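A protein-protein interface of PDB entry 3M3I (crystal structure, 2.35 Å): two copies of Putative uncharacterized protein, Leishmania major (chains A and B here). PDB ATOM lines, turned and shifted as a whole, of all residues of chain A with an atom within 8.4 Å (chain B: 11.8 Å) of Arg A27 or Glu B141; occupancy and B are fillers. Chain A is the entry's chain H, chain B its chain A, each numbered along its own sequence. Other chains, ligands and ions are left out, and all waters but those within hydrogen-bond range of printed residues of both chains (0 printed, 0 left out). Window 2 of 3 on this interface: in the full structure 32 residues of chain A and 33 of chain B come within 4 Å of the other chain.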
ATOM      1  N   ASN A  19      -0.994 -10.896  14.641  1.00  0.00           N
ATOM      2  CA  ASN A  19      -0.508 -12.205  14.200  1.00  0.00           C
ATOM      3  C   ASN A  19      -1.656 -12.983  13.599  1.00  0.00           C
ATOM      4  O   ASN A  19      -2.799 -12.872  14.040  1.00  0.00           O
ATOM      5  CB  ASN A  19       0.107 -12.999  15.350  1.00  0.00           C
ATOM      6  CG  ASN A  19       1.571 -12.667  15.586  1.00  0.00           C
ATOM      7  OD1 ASN A  19       2.239 -12.070  14.726  1.00  0.00           O
ATOM      8  ND2 ASN A  19       2.080 -13.053  16.757  1.00  0.00           N
ATOM      9  N   THR A  20      -1.321 -13.789  12.600  1.00  0.00           N
ATOM     10  CA  THR A  20      -2.291 -14.404  11.716  1.00  0.00           C
ATOM     11  C   THR A  20      -2.013 -15.912  11.731  1.00  0.00           C
ATOM     12  O   THR A  20      -0.957 -16.336  12.201  1.00  0.00           O
ATOM     13  CB  THR A  20      -2.143 -13.781  10.296  1.00  0.00           C
ATOM     14  OG1 THR A  20      -3.276 -14.106   9.470  1.00  0.00           O
ATOM     15  CG2 THR A  20      -0.854 -14.248   9.624  1.00  0.00           C
ATOM     16  N   ALA A  21      -2.960 -16.722  11.266  1.00  0.00           N
ATOM     17  CA  ALA A  21      -2.749 -18.170  11.206  1.00  0.00           C
ATOM     18  C   ALA A  21      -1.434 -18.537  10.491  1.00  0.00           C
ATOM     19  O   ALA A  21      -0.711 -19.418  10.956  1.00  0.00           O
ATOM     20  CB  ALA A  21      -3.937 -18.864  10.542  1.00  0.00           C
ATOM     21  N   GLU A  22      -1.124 -17.847   9.390  1.00  0.00           N
ATOM     22  CA  GLU A  22       0.069 -18.131   8.586  1.00  0.00           C
ATOM     23  C   GLU A  22       1.377 -17.734   9.318  1.00  0.00           C
ATOM     24  O   GLU A  22       2.418 -18.361   9.108  1.00  0.00           O
ATOM     25  CB  GLU A  22      -0.047 -17.499   7.170  1.00  0.00           C
ATOM     26  CG  GLU A  22      -1.326 -17.964   6.363  1.00  0.00           C
ATOM     27  CD  GLU A  22      -1.373 -17.560   4.859  1.00  0.00           C
ATOM     28  OE1 GLU A  22      -1.386 -16.347   4.522  1.00  0.00           O
ATOM     29  OE2 GLU A  22      -1.458 -18.474   3.995  1.00  0.00           O
ATOM     30  N   PHE A  23       1.318 -16.737  10.203  1.00  0.00           N
ATOM     31  CA  PHE A  23       2.489 -16.331  10.999  1.00  0.00           C
ATOM     32  C   PHE A  23       2.971 -17.527  11.784  1.00  0.00           C
ATOM     33  O   PHE A  23       4.148 -17.892  11.698  1.00  0.00           O
ATOM     34  CB  PHE A  23       2.142 -15.181  11.961  1.00  0.00           C
ATOM     35  CG  PHE A  23       3.183 -14.914  13.034  1.00  0.00           C
ATOM     36  CD1 PHE A  23       3.079 -15.498  14.284  1.00  0.00           C
ATOM     37  CD2 PHE A  23       4.243 -14.057  12.799  1.00  0.00           C
ATOM     38  CE1 PHE A  23       4.028 -15.259  15.278  1.00  0.00           C
ATOM     39  CE2 PHE A  23       5.193 -13.795  13.793  1.00  0.00           C
ATOM     40  CZ  PHE A  23       5.082 -14.407  15.035  1.00  0.00           C
ATOM     41  N   TRP A  24       2.041 -18.137  12.530  1.00  0.00           N
ATOM     42  CA  TRP A  24       2.340 -19.260  13.409  1.00  0.00           C
ATOM     43  C   TRP A  24       2.727 -20.495  12.628  1.00  0.00           C
ATOM     44  O   TRP A  24       3.766 -21.085  12.906  1.00  0.00           O
ATOM     45  CB  TRP A  24       1.157 -19.576  14.337  1.00  0.00           C
ATOM     46  CG  TRP A  24       0.888 -18.474  15.291  1.00  0.00           C
ATOM     47  CD1 TRP A  24      -0.196 -17.636  15.309  1.00  0.00           C
ATOM     48  CD2 TRP A  24       1.737 -18.051  16.358  1.00  0.00           C
ATOM     49  NE1 TRP A  24      -0.075 -16.728  16.331  1.00  0.00           N
ATOM     50  CE2 TRP A  24       1.097 -16.969  16.998  1.00  0.00           C
ATOM     51  CE3 TRP A  24       2.971 -18.489  16.841  1.00  0.00           C
ATOM     52  CZ2 TRP A  24       1.655 -16.316  18.099  1.00  0.00           C
ATOM     53  CZ3 TRP A  24       3.513 -17.855  17.935  1.00  0.00           C
ATOM     54  CH2 TRP A  24       2.863 -16.768  18.549  1.00  0.00           C
ATOM     55  N   ILE A  25       1.912 -20.874  11.640  1.00  0.00           N
ATOM     56  CA  ILE A  25       2.163 -22.106  10.871  1.00  0.00           C
ATOM     57  C   ILE A  25       3.594 -22.072  10.367  1.00  0.00           C
ATOM     58  O   ILE A  25       4.292 -23.076  10.356  1.00  0.00           O
ATOM     59  CB  ILE A  25       1.187 -22.251   9.674  1.00  0.00           C
ATOM     60  CG1 ILE A  25      -0.242 -22.514  10.164  1.00  0.00           C
ATOM     61  CG2 ILE A  25       1.619 -23.373   8.735  1.00  0.00           C
ATOM     62  CD1 ILE A  25      -1.300 -22.181   9.137  1.00  0.00           C
ATOM     63  N   LYS A  26       4.036 -20.893   9.969  1.00  0.00           N
ATOM     64  CA  LYS A  26       5.373 -20.722   9.433  1.00  0.00           C
ATOM     65  C   LYS A  26       6.408 -20.804  10.558  1.00  0.00           C
ATOM     66  O   LYS A  26       7.421 -21.494  10.442  1.00  0.00           O
ATOM     67  CB  LYS A  26       5.461 -19.383   8.681  1.00  0.00           C
ATOM     68  CG  LYS A  26       6.701 -19.198   7.839  1.00  0.00           C
ATOM     69  CD  LYS A  26       6.481 -18.089   6.786  1.00  0.00           C
ATOM     70  CE  LYS A  26       7.784 -17.396   6.322  1.00  0.00           C
ATOM     71  NZ  LYS A  26       7.928 -16.004   6.897  1.00  0.00           N
ATOM     72  N   ARG A  27       6.142 -20.126  11.664  1.00  0.00           N
ATOM     73  CA  ARG A  27       7.180 -19.978  12.679  1.00  0.00           C
ATOM     74  C   ARG A  27       7.361 -21.200  13.560  1.00  0.00           C
ATOM     75  O   ARG A  27       8.484 -21.545  13.915  1.00  0.00           O
ATOM     76  CB  ARG A  27       6.996 -18.676  13.467  1.00  0.00           C
ATOM     77  CG  ARG A  27       7.743 -17.534  12.758  1.00  0.00           C
ATOM     78  CD  ARG A  27       7.410 -16.187  13.292  1.00  0.00           C
ATOM     79  NE  ARG A  27       7.985 -15.103  12.489  1.00  0.00           N
ATOM     80  CZ  ARG A  27       9.265 -14.716  12.507  1.00  0.00           C
ATOM     81  NH1 ARG A  27      10.179 -15.337  13.260  1.00  0.00           N
ATOM     82  NH2 ARG A  27       9.649 -13.691  11.744  1.00  0.00           N
ATOM     83  N   LEU A  28       6.271 -21.896  13.847  1.00  0.00           N
ATOM     84  CA  LEU A  28       6.347 -23.167  14.570  1.00  0.00           C
ATOM     85  C   LEU A  28       6.560 -24.397  13.667  1.00  0.00           C
ATOM     86  O   LEU A  28       6.627 -25.511  14.177  1.00  0.00           O
ATOM     87  CB  LEU A  28       5.085 -23.354  15.430  1.00  0.00           C
ATOM     88  CG  LEU A  28       4.792 -22.237  16.428  1.00  0.00           C
ATOM     89  CD1 LEU A  28       3.561 -22.541  17.237  1.00  0.00           C
ATOM     90  CD2 LEU A  28       5.984 -22.020  17.328  1.00  0.00           C
ATOM     91  N   GLN A  29       6.673 -24.195  12.350  1.00  0.00           N
ATOM     92  CA  GLN A  29       6.818 -25.295  11.354  1.00  0.00           C
ATOM     93  C   GLN A  29       5.704 -26.348  11.438  1.00  0.00           C
ATOM     94  O   GLN A  29       5.976 -27.540  11.452  1.00  0.00           O
ATOM     95  CB  GLN A  29       8.193 -25.979  11.473  1.00  0.00           C
ATOM     96  CG  GLN A  29       9.390 -25.060  11.223  1.00  0.00           C
ATOM     97  CD  GLN A  29      10.728 -25.650  11.693  1.00  0.00           C
ATOM     98  OE1 GLN A  29      11.029 -26.825  11.462  1.00  0.00           O
ATOM     99  NE2 GLN A  29      11.537 -24.823  12.348  1.00  0.00           N
ATOM    100  N   LEU A  30       4.453 -25.896  11.477  1.00  0.00           N
ATOM    101  CA  LEU A  30       3.306 -26.780  11.684  1.00  0.00           C
ATOM    102  C   LEU A  30       2.854 -27.367  10.359  1.00  0.00           C
ATOM    103  O   LEU A  30       2.974 -26.714   9.331  1.00  0.00           O
ATOM    104  CB  LEU A  30       2.137 -26.028  12.329  1.00  0.00           C
ATOM    105  CG  LEU A  30       2.390 -25.257  13.632  1.00  0.00           C
ATOM    106  CD1 LEU A  30       1.087 -24.700  14.171  1.00  0.00           C
ATOM    107  CD2 LEU A  30       3.053 -26.111  14.696  1.00  0.00           C
ATOM    108  N   SER A  40       2.384 -29.874  15.394  1.00  0.00           N
ATOM    109  CA  SER A  40       3.781 -30.297  15.325  1.00  0.00           C
ATOM    110  C   SER A  40       4.172 -30.953  16.652  1.00  0.00           C
ATOM    111  O   SER A  40       3.911 -30.408  17.719  1.00  0.00           O
ATOM    112  CB  SER A  40       4.698 -29.116  15.023  1.00  0.00           C
ATOM    113  OG  SER A  40       6.050 -29.456  15.210  1.00  0.00           O
ATOM    114  N   TYR A  64       2.248 -28.719  19.637  1.00  0.00           N
ATOM    115  CA  TYR A  64       1.540 -27.502  19.315  1.00  0.00           C
ATOM    116  C   TYR A  64       0.346 -27.876  18.448  1.00  0.00           C
ATOM    117  O   TYR A  64       0.444 -28.744  17.579  1.00  0.00           O
ATOM    118  CB  TYR A  64       2.427 -26.542  18.558  1.00  0.00           C
ATOM    119  CG  TYR A  64       3.603 -26.041  19.343  1.00  0.00           C
ATOM    120  CD1 TYR A  64       3.430 -25.277  20.489  1.00  0.00           C
ATOM    121  CD2 TYR A  64       4.899 -26.302  18.922  1.00  0.00           C
ATOM    122  CE1 TYR A  64       4.519 -24.803  21.195  1.00  0.00           C
ATOM    123  CE2 TYR A  64       5.993 -25.829  19.624  1.00  0.00           C
ATOM    124  CZ  TYR A  64       5.797 -25.088  20.752  1.00  0.00           C
ATOM    125  OH  TYR A  64       6.890 -24.644  21.427  1.00  0.00           O
ATOM    126  N   TYR B  86       3.403 -21.054  28.273  1.00  0.00           N
ATOM    127  CA  TYR B  86       3.092 -19.637  28.415  1.00  0.00           C
ATOM    128  C   TYR B  86       1.589 -19.304  28.205  1.00  0.00           C
ATOM    129  O   TYR B  86       0.985 -19.733  27.234  1.00  0.00           O
ATOM    130  CB  TYR B  86       3.937 -18.807  27.436  1.00  0.00           C
ATOM    131  CG  TYR B  86       3.552 -17.343  27.408  1.00  0.00           C
ATOM    132  CD1 TYR B  86       2.499 -16.896  26.602  1.00  0.00           C
ATOM    133  CD2 TYR B  86       4.217 -16.405  28.207  1.00  0.00           C
ATOM    134  CE1 TYR B  86       2.135 -15.555  26.569  1.00  0.00           C
ATOM    135  CE2 TYR B  86       3.856 -15.046  28.184  1.00  0.00           C
ATOM    136  CZ  TYR B  86       2.807 -14.636  27.370  1.00  0.00           C
ATOM    137  OH  TYR B  86       2.417 -13.324  27.344  1.00  0.00           O
ATOM    138  N   PRO B  91       7.535 -12.654  29.395  1.00  0.00           N
ATOM    139  CA  PRO B  91       8.268 -13.910  29.319  1.00  0.00           C
ATOM    140  C   PRO B  91       8.828 -14.328  30.650  1.00  0.00           C
ATOM    141  O   PRO B  91       9.256 -13.483  31.435  1.00  0.00           O
ATOM    142  CB  PRO B  91       9.432 -13.603  28.368  1.00  0.00           C
ATOM    143  CG  PRO B  91       9.449 -12.155  28.191  1.00  0.00           C
ATOM    144  CD  PRO B  91       8.042 -11.689  28.410  1.00  0.00           C
ATOM    145  N   LEU B 135      13.806 -18.423  27.731  1.00  0.00           N
ATOM    146  CA  LEU B 135      12.661 -17.529  27.893  1.00  0.00           C
ATOM    147  C   LEU B 135      11.413 -18.256  27.439  1.00  0.00           C
ATOM    148  O   LEU B 135      11.308 -18.577  26.289  1.00  0.00           O
ATOM    149  CB  LEU B 135      12.830 -16.265  27.060  1.00  0.00           C
ATOM    150  CG  LEU B 135      13.904 -15.276  27.520  1.00  0.00           C
ATOM    151  CD1 LEU B 135      14.309 -14.352  26.379  1.00  0.00           C
ATOM    152  CD2 LEU B 135      13.420 -14.484  28.702  1.00  0.00           C
ATOM    153  N   VAL B 136      10.485 -18.528  28.351  1.00  0.00           N
ATOM    154  CA  VAL B 136       9.163 -19.065  28.006  1.00  0.00           C
ATOM    155  C   VAL B 136       8.260 -17.873  27.729  1.00  0.00           C
ATOM    156  O   VAL B 136       8.015 -17.061  28.621  1.00  0.00           O
ATOM    157  CB  VAL B 136       8.585 -19.916  29.173  1.00  0.00           C
ATOM    158  CG1 VAL B 136       7.097 -20.283  28.925  1.00  0.00           C
ATOM    159  CG2 VAL B 136       9.423 -21.159  29.362  1.00  0.00           C
ATOM    160  N   GLY B 137       7.789 -17.745  26.489  1.00  0.00           N
ATOM    161  CA  GLY B 137       7.050 -16.531  26.082  1.00  0.00           C
ATOM    162  C   GLY B 137       6.399 -16.663  24.717  1.00  0.00           C
ATOM    163  O   GLY B 137       6.487 -17.724  24.091  1.00  0.00           O
ATOM    164  N   ALA B 138       5.755 -15.586  24.263  1.00  0.00           N
ATOM    165  CA  ALA B 138       4.956 -15.597  23.028  1.00  0.00           C
ATOM    166  C   ALA B 138       5.560 -14.799  21.863  1.00  0.00           C
ATOM    167  O   ALA B 138       4.988 -14.766  20.772  1.00  0.00           O
ATOM    168  CB  ALA B 138       3.538 -15.087  23.320  1.00  0.00           C
ATOM    169  N   ARG B 139       6.681 -14.118  22.091  1.00  0.00           N
ATOM    170  CA  ARG B 139       7.404 -13.505  20.996  1.00  0.00           C
ATOM    171  C   ARG B 139       8.481 -14.472  20.579  1.00  0.00           C
ATOM    172  O   ARG B 139       9.657 -14.339  20.942  1.00  0.00           O
ATOM    173  CB  ARG B 139       8.000 -12.161  21.391  1.00  0.00           C
ATOM    174  CG  ARG B 139       6.965 -11.079  21.641  1.00  0.00           C
ATOM    175  CD  ARG B 139       7.453 -10.172  22.752  1.00  0.00           C
ATOM    176  NE  ARG B 139       6.708  -8.922  22.876  1.00  0.00           N
ATOM    177  CZ  ARG B 139       6.931  -8.025  23.832  1.00  0.00           C
ATOM    178  NH1 ARG B 139       7.875  -8.239  24.752  1.00  0.00           N
ATOM    179  NH2 ARG B 139       6.210  -6.916  23.881  1.00  0.00           N
ATOM    180  N   VAL B 140       8.056 -15.450  19.793  1.00  0.00           N
ATOM    181  CA  VAL B 140       8.951 -16.490  19.278  1.00  0.00           C
ATOM    182  C   VAL B 140       9.961 -15.949  18.279  1.00  0.00           C
ATOM    183  O   VAL B 140      10.995 -16.578  18.051  1.00  0.00           O
ATOM    184  CB  VAL B 140       8.171 -17.615  18.616  1.00  0.00           C
ATOM    185  CG1 VAL B 140       7.271 -18.309  19.676  1.00  0.00           C
ATOM    186  CG2 VAL B 140       7.383 -17.075  17.420  1.00  0.00           C
ATOM    187  N   GLU B 141       9.664 -14.785  17.711  1.00  0.00           N
ATOM    188  CA  GLU B 141      10.573 -14.108  16.807  1.00  0.00           C
ATOM    189  C   GLU B 141      11.740 -13.448  17.540  1.00  0.00           C
ATOM    190  O   GLU B 141      12.680 -12.988  16.908  1.00  0.00           O
ATOM    191  CB  GLU B 141       9.804 -13.129  15.889  1.00  0.00           C
ATOM    192  CG  GLU B 141       9.142 -11.911  16.550  1.00  0.00           C
ATOM    193  CD  GLU B 141       7.865 -12.204  17.357  1.00  0.00           C
ATOM    194  OE1 GLU B 141       7.144 -11.237  17.654  1.00  0.00           O
ATOM    195  OE2 GLU B 141       7.594 -13.365  17.737  1.00  0.00           O
ATOM    196  N   ARG B 142      11.661 -13.411  18.874  1.00  0.00           N
ATOM    197  CA  ARG B 142      12.752 -12.995  19.775  1.00  0.00           C
ATOM    198  C   ARG B 142      13.355 -14.174  20.561  1.00  0.00           C
ATOM    199  O   ARG B 142      13.992 -13.975  21.582  1.00  0.00           O
ATOM    200  CB  ARG B 142      12.225 -11.998  20.790  1.00  0.00           C
ATOM    201  CG  ARG B 142      11.789 -10.693  20.230  1.00  0.00           C
ATOM    202  CD  ARG B 142      11.267  -9.839  21.354  1.00  0.00           C
ATOM    203  NE  ARG B 142      11.024  -8.467  20.940  1.00  0.00           N
ATOM    204  CZ  ARG B 142      10.499  -7.533  21.719  1.00  0.00           C
ATOM    205  NH1 ARG B 142      10.147  -7.831  22.966  1.00  0.00           N
ATOM    206  NH2 ARG B 142      10.326  -6.296  21.253  1.00  0.00           N
ATOM    207  N   GLY B 143      13.141 -15.399  20.103  1.00  0.00           N
ATOM    208  CA  GLY B 143      13.729 -16.550  20.754  1.00  0.00           C
ATOM    209  C   GLY B 143      12.962 -17.072  21.955  1.00  0.00           C
ATOM    210  O   GLY B 143      13.429 -17.990  22.624  1.00  0.00           O
ATOM    211  N   GLU B 144      11.784 -16.516  22.226  1.00  0.00           N
ATOM    212  CA  GLU B 144      10.953 -17.011  23.309  1.00  0.00           C
ATOM    213  C   GLU B 144      10.280 -18.291  22.844  1.00  0.00           C
ATOM    214  O   GLU B 144      10.109 -18.481  21.661  1.00  0.00           O
ATOM    215  CB  GLU B 144       9.916 -15.968  23.746  1.00  0.00           C
ATOM    216  CG  GLU B 144      10.542 -14.648  24.214  1.00  0.00           C
ATOM    217  CD  GLU B 144       9.517 -13.569  24.492  1.00  0.00           C
ATOM    218  OE1 GLU B 144       8.304 -13.877  24.440  1.00  0.00           O
ATOM    219  OE2 GLU B 144       9.925 -12.410  24.745  1.00  0.00           O
ATOM    220  N   LEU B 145       9.922 -19.162  23.791  1.00  0.00           N
ATOM    221  CA  LEU B 145       9.330 -20.462  23.494  1.00  0.00           C
ATOM    222  C   LEU B 145       8.002 -20.631  24.219  1.00  0.00           C
ATOM    223  O   LEU B 145       7.967 -20.595  25.440  1.00  0.00           O
ATOM    224  CB  LEU B 145      10.297 -21.559  23.916  1.00  0.00           C
ATOM    225  CG  LEU B 145      11.658 -21.593  23.204  1.00  0.00           C
ATOM    226  CD1 LEU B 145      12.626 -22.606  23.841  1.00  0.00           C
ATOM    227  CD2 LEU B 145      11.499 -21.867  21.727  1.00  0.00           C
ATOM    228  N   LEU B 146       6.909 -20.818  23.487  1.00  0.00           N
ATOM    229  CA  LEU B 146       5.591 -20.974  24.090  1.00  0.00           C
ATOM    230  C   LEU B 146       5.506 -22.165  25.024  1.00  0.00           C
ATOM    231  O   LEU B 146       4.705 -22.181  25.951  1.00  0.00           O
ATOM    232  CB  LEU B 146       4.519 -21.138  23.025  1.00  0.00           C
ATOM    233  CG  LEU B 146       4.078 -19.939  22.191  1.00  0.00           C
ATOM    234  CD1 LEU B 146       3.242 -20.460  21.057  1.00  0.00           C
ATOM    235  CD2 LEU B 146       3.306 -18.892  23.018  1.00  0.00           C
ATOM    236  N   GLN B 147       6.336 -23.166  24.765  1.00  0.00           N
ATOM    237  CA  GLN B 147       6.388 -24.392  25.553  1.00  0.00           C
ATOM    238  C   GLN B 147       7.860 -24.780  25.724  1.00  0.00           C
ATOM    239  O   GLN B 147       8.667 -24.548  24.841  1.00  0.00           O
ATOM    240  CB  GLN B 147       5.604 -25.470  24.798  1.00  0.00           C
ATOM    241  CG  GLN B 147       5.497 -26.817  25.474  1.00  0.00           C
ATOM    242  CD  GLN B 147       5.120 -27.947  24.517  1.00  0.00           C
ATOM    243  OE1 GLN B 147       5.645 -29.027  24.623  1.00  0.00           O
ATOM    244  NE2 GLN B 147       4.181 -27.700  23.611  1.00  0.00           N
ATOM    245  N   ALA B 165      12.362  -4.515  27.722  1.00  0.00           N
ATOM    246  CA  ALA B 165      11.421  -5.251  26.853  1.00  0.00           C
ATOM    247  C   ALA B 165      10.790  -6.487  27.515  1.00  0.00           C
ATOM    248  O   ALA B 165       9.631  -6.802  27.245  1.00  0.00           O
ATOM    249  CB  ALA B 165      12.112  -5.650  25.548  1.00  0.00           C
ATOM    250  N   ASP B 166      11.551  -7.178  28.363  1.00  0.00           N
ATOM    251  CA  ASP B 166      11.083  -8.389  29.046  1.00  0.00           C
ATOM    252  C   ASP B 166      10.350  -8.122  30.371  1.00  0.00           C
ATOM    253  O   ASP B 166       9.947  -9.076  31.056  1.00  0.00           O
ATOM    254  CB  ASP B 166      12.270  -9.308  29.360  1.00  0.00           C
ATOM    255  CG  ASP B 166      12.935  -9.877  28.122  1.00  0.00           C
ATOM    256  OD1 ASP B 166      12.949  -9.205  27.065  1.00  0.00           O
ATOM    257  OD2 ASP B 166      13.473 -11.004  28.231  1.00  0.00           O
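N of Ala B138 is in hydrogen-bond range of OE1 of Glu B144, 3.1 Å away. The backbone NH of Tyr A64 sits at hydrogen-bond distance from the backbone carbonyl oxygen of Ser A40 (3.0 Å).
Along chain B the printed residues that touch a printed residue of chain A span positions 138 to 147. Printed residues of chain A that touch a printed residue of chain B: Phe A23, Trp A24, Arg A27 and Tyr A64. Hydrophobic or aromatic side chains of chain A that line the printed part of chain B: Phe A23, Trp A24 and Tyr A64. Along chain A the printed residues that touch a printed residue of chain B span positions 23 to 64. Among the printed residues, no Asp or Glu carboxylate lies within 4 Å of a Lys or Arg side-chain nitrogen of the other chain.
Glu B141 touches Phe A23. O of Ala B138 touches CH2 of Trp A24, at 3.7 Å. CG2 of Val B140 touches CZ3 of Trp A24, 3.98 Å away. NH1 of Arg A27 touches CB of Glu B141 (3.5 Å). Tyr A64 touches Gln B147.
No position is printed for both chains. Of the 5 pairs that touch across the chains among the printed residues, none has its exchanged pair printed and touching as well.
Of chain A, only Phe A23 (3.8 Å) and Arg A27 (3.5 Å) come within 4 Å of Glu B141. No residue of chain B comes within 4 Å of Lys A26. No residue of chain B comes within 4 Å of Leu A28. Printed residues of chain B within 4 Å of Trp A24: Ala B138 (3.7 Å) and Val B140 (3.98 Å). Printed residues of chain A within 4 Å of Ala B138: Trp A24 (3.7 Å). Of the printed residues of chain A, Gln B147 touches Tyr A64. Of the printed residues of chain A, Val B140 touches Trp A24 (3.98 Å). Val B136 touches none of the printed residues of chain A. The nearest residue of chain A that does not touch Glu B141 is Asn A19 (5.5 Å). The nearest printed residue of chain B that does not touch Tyr A64 is Leu B146 (4.1 Å).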
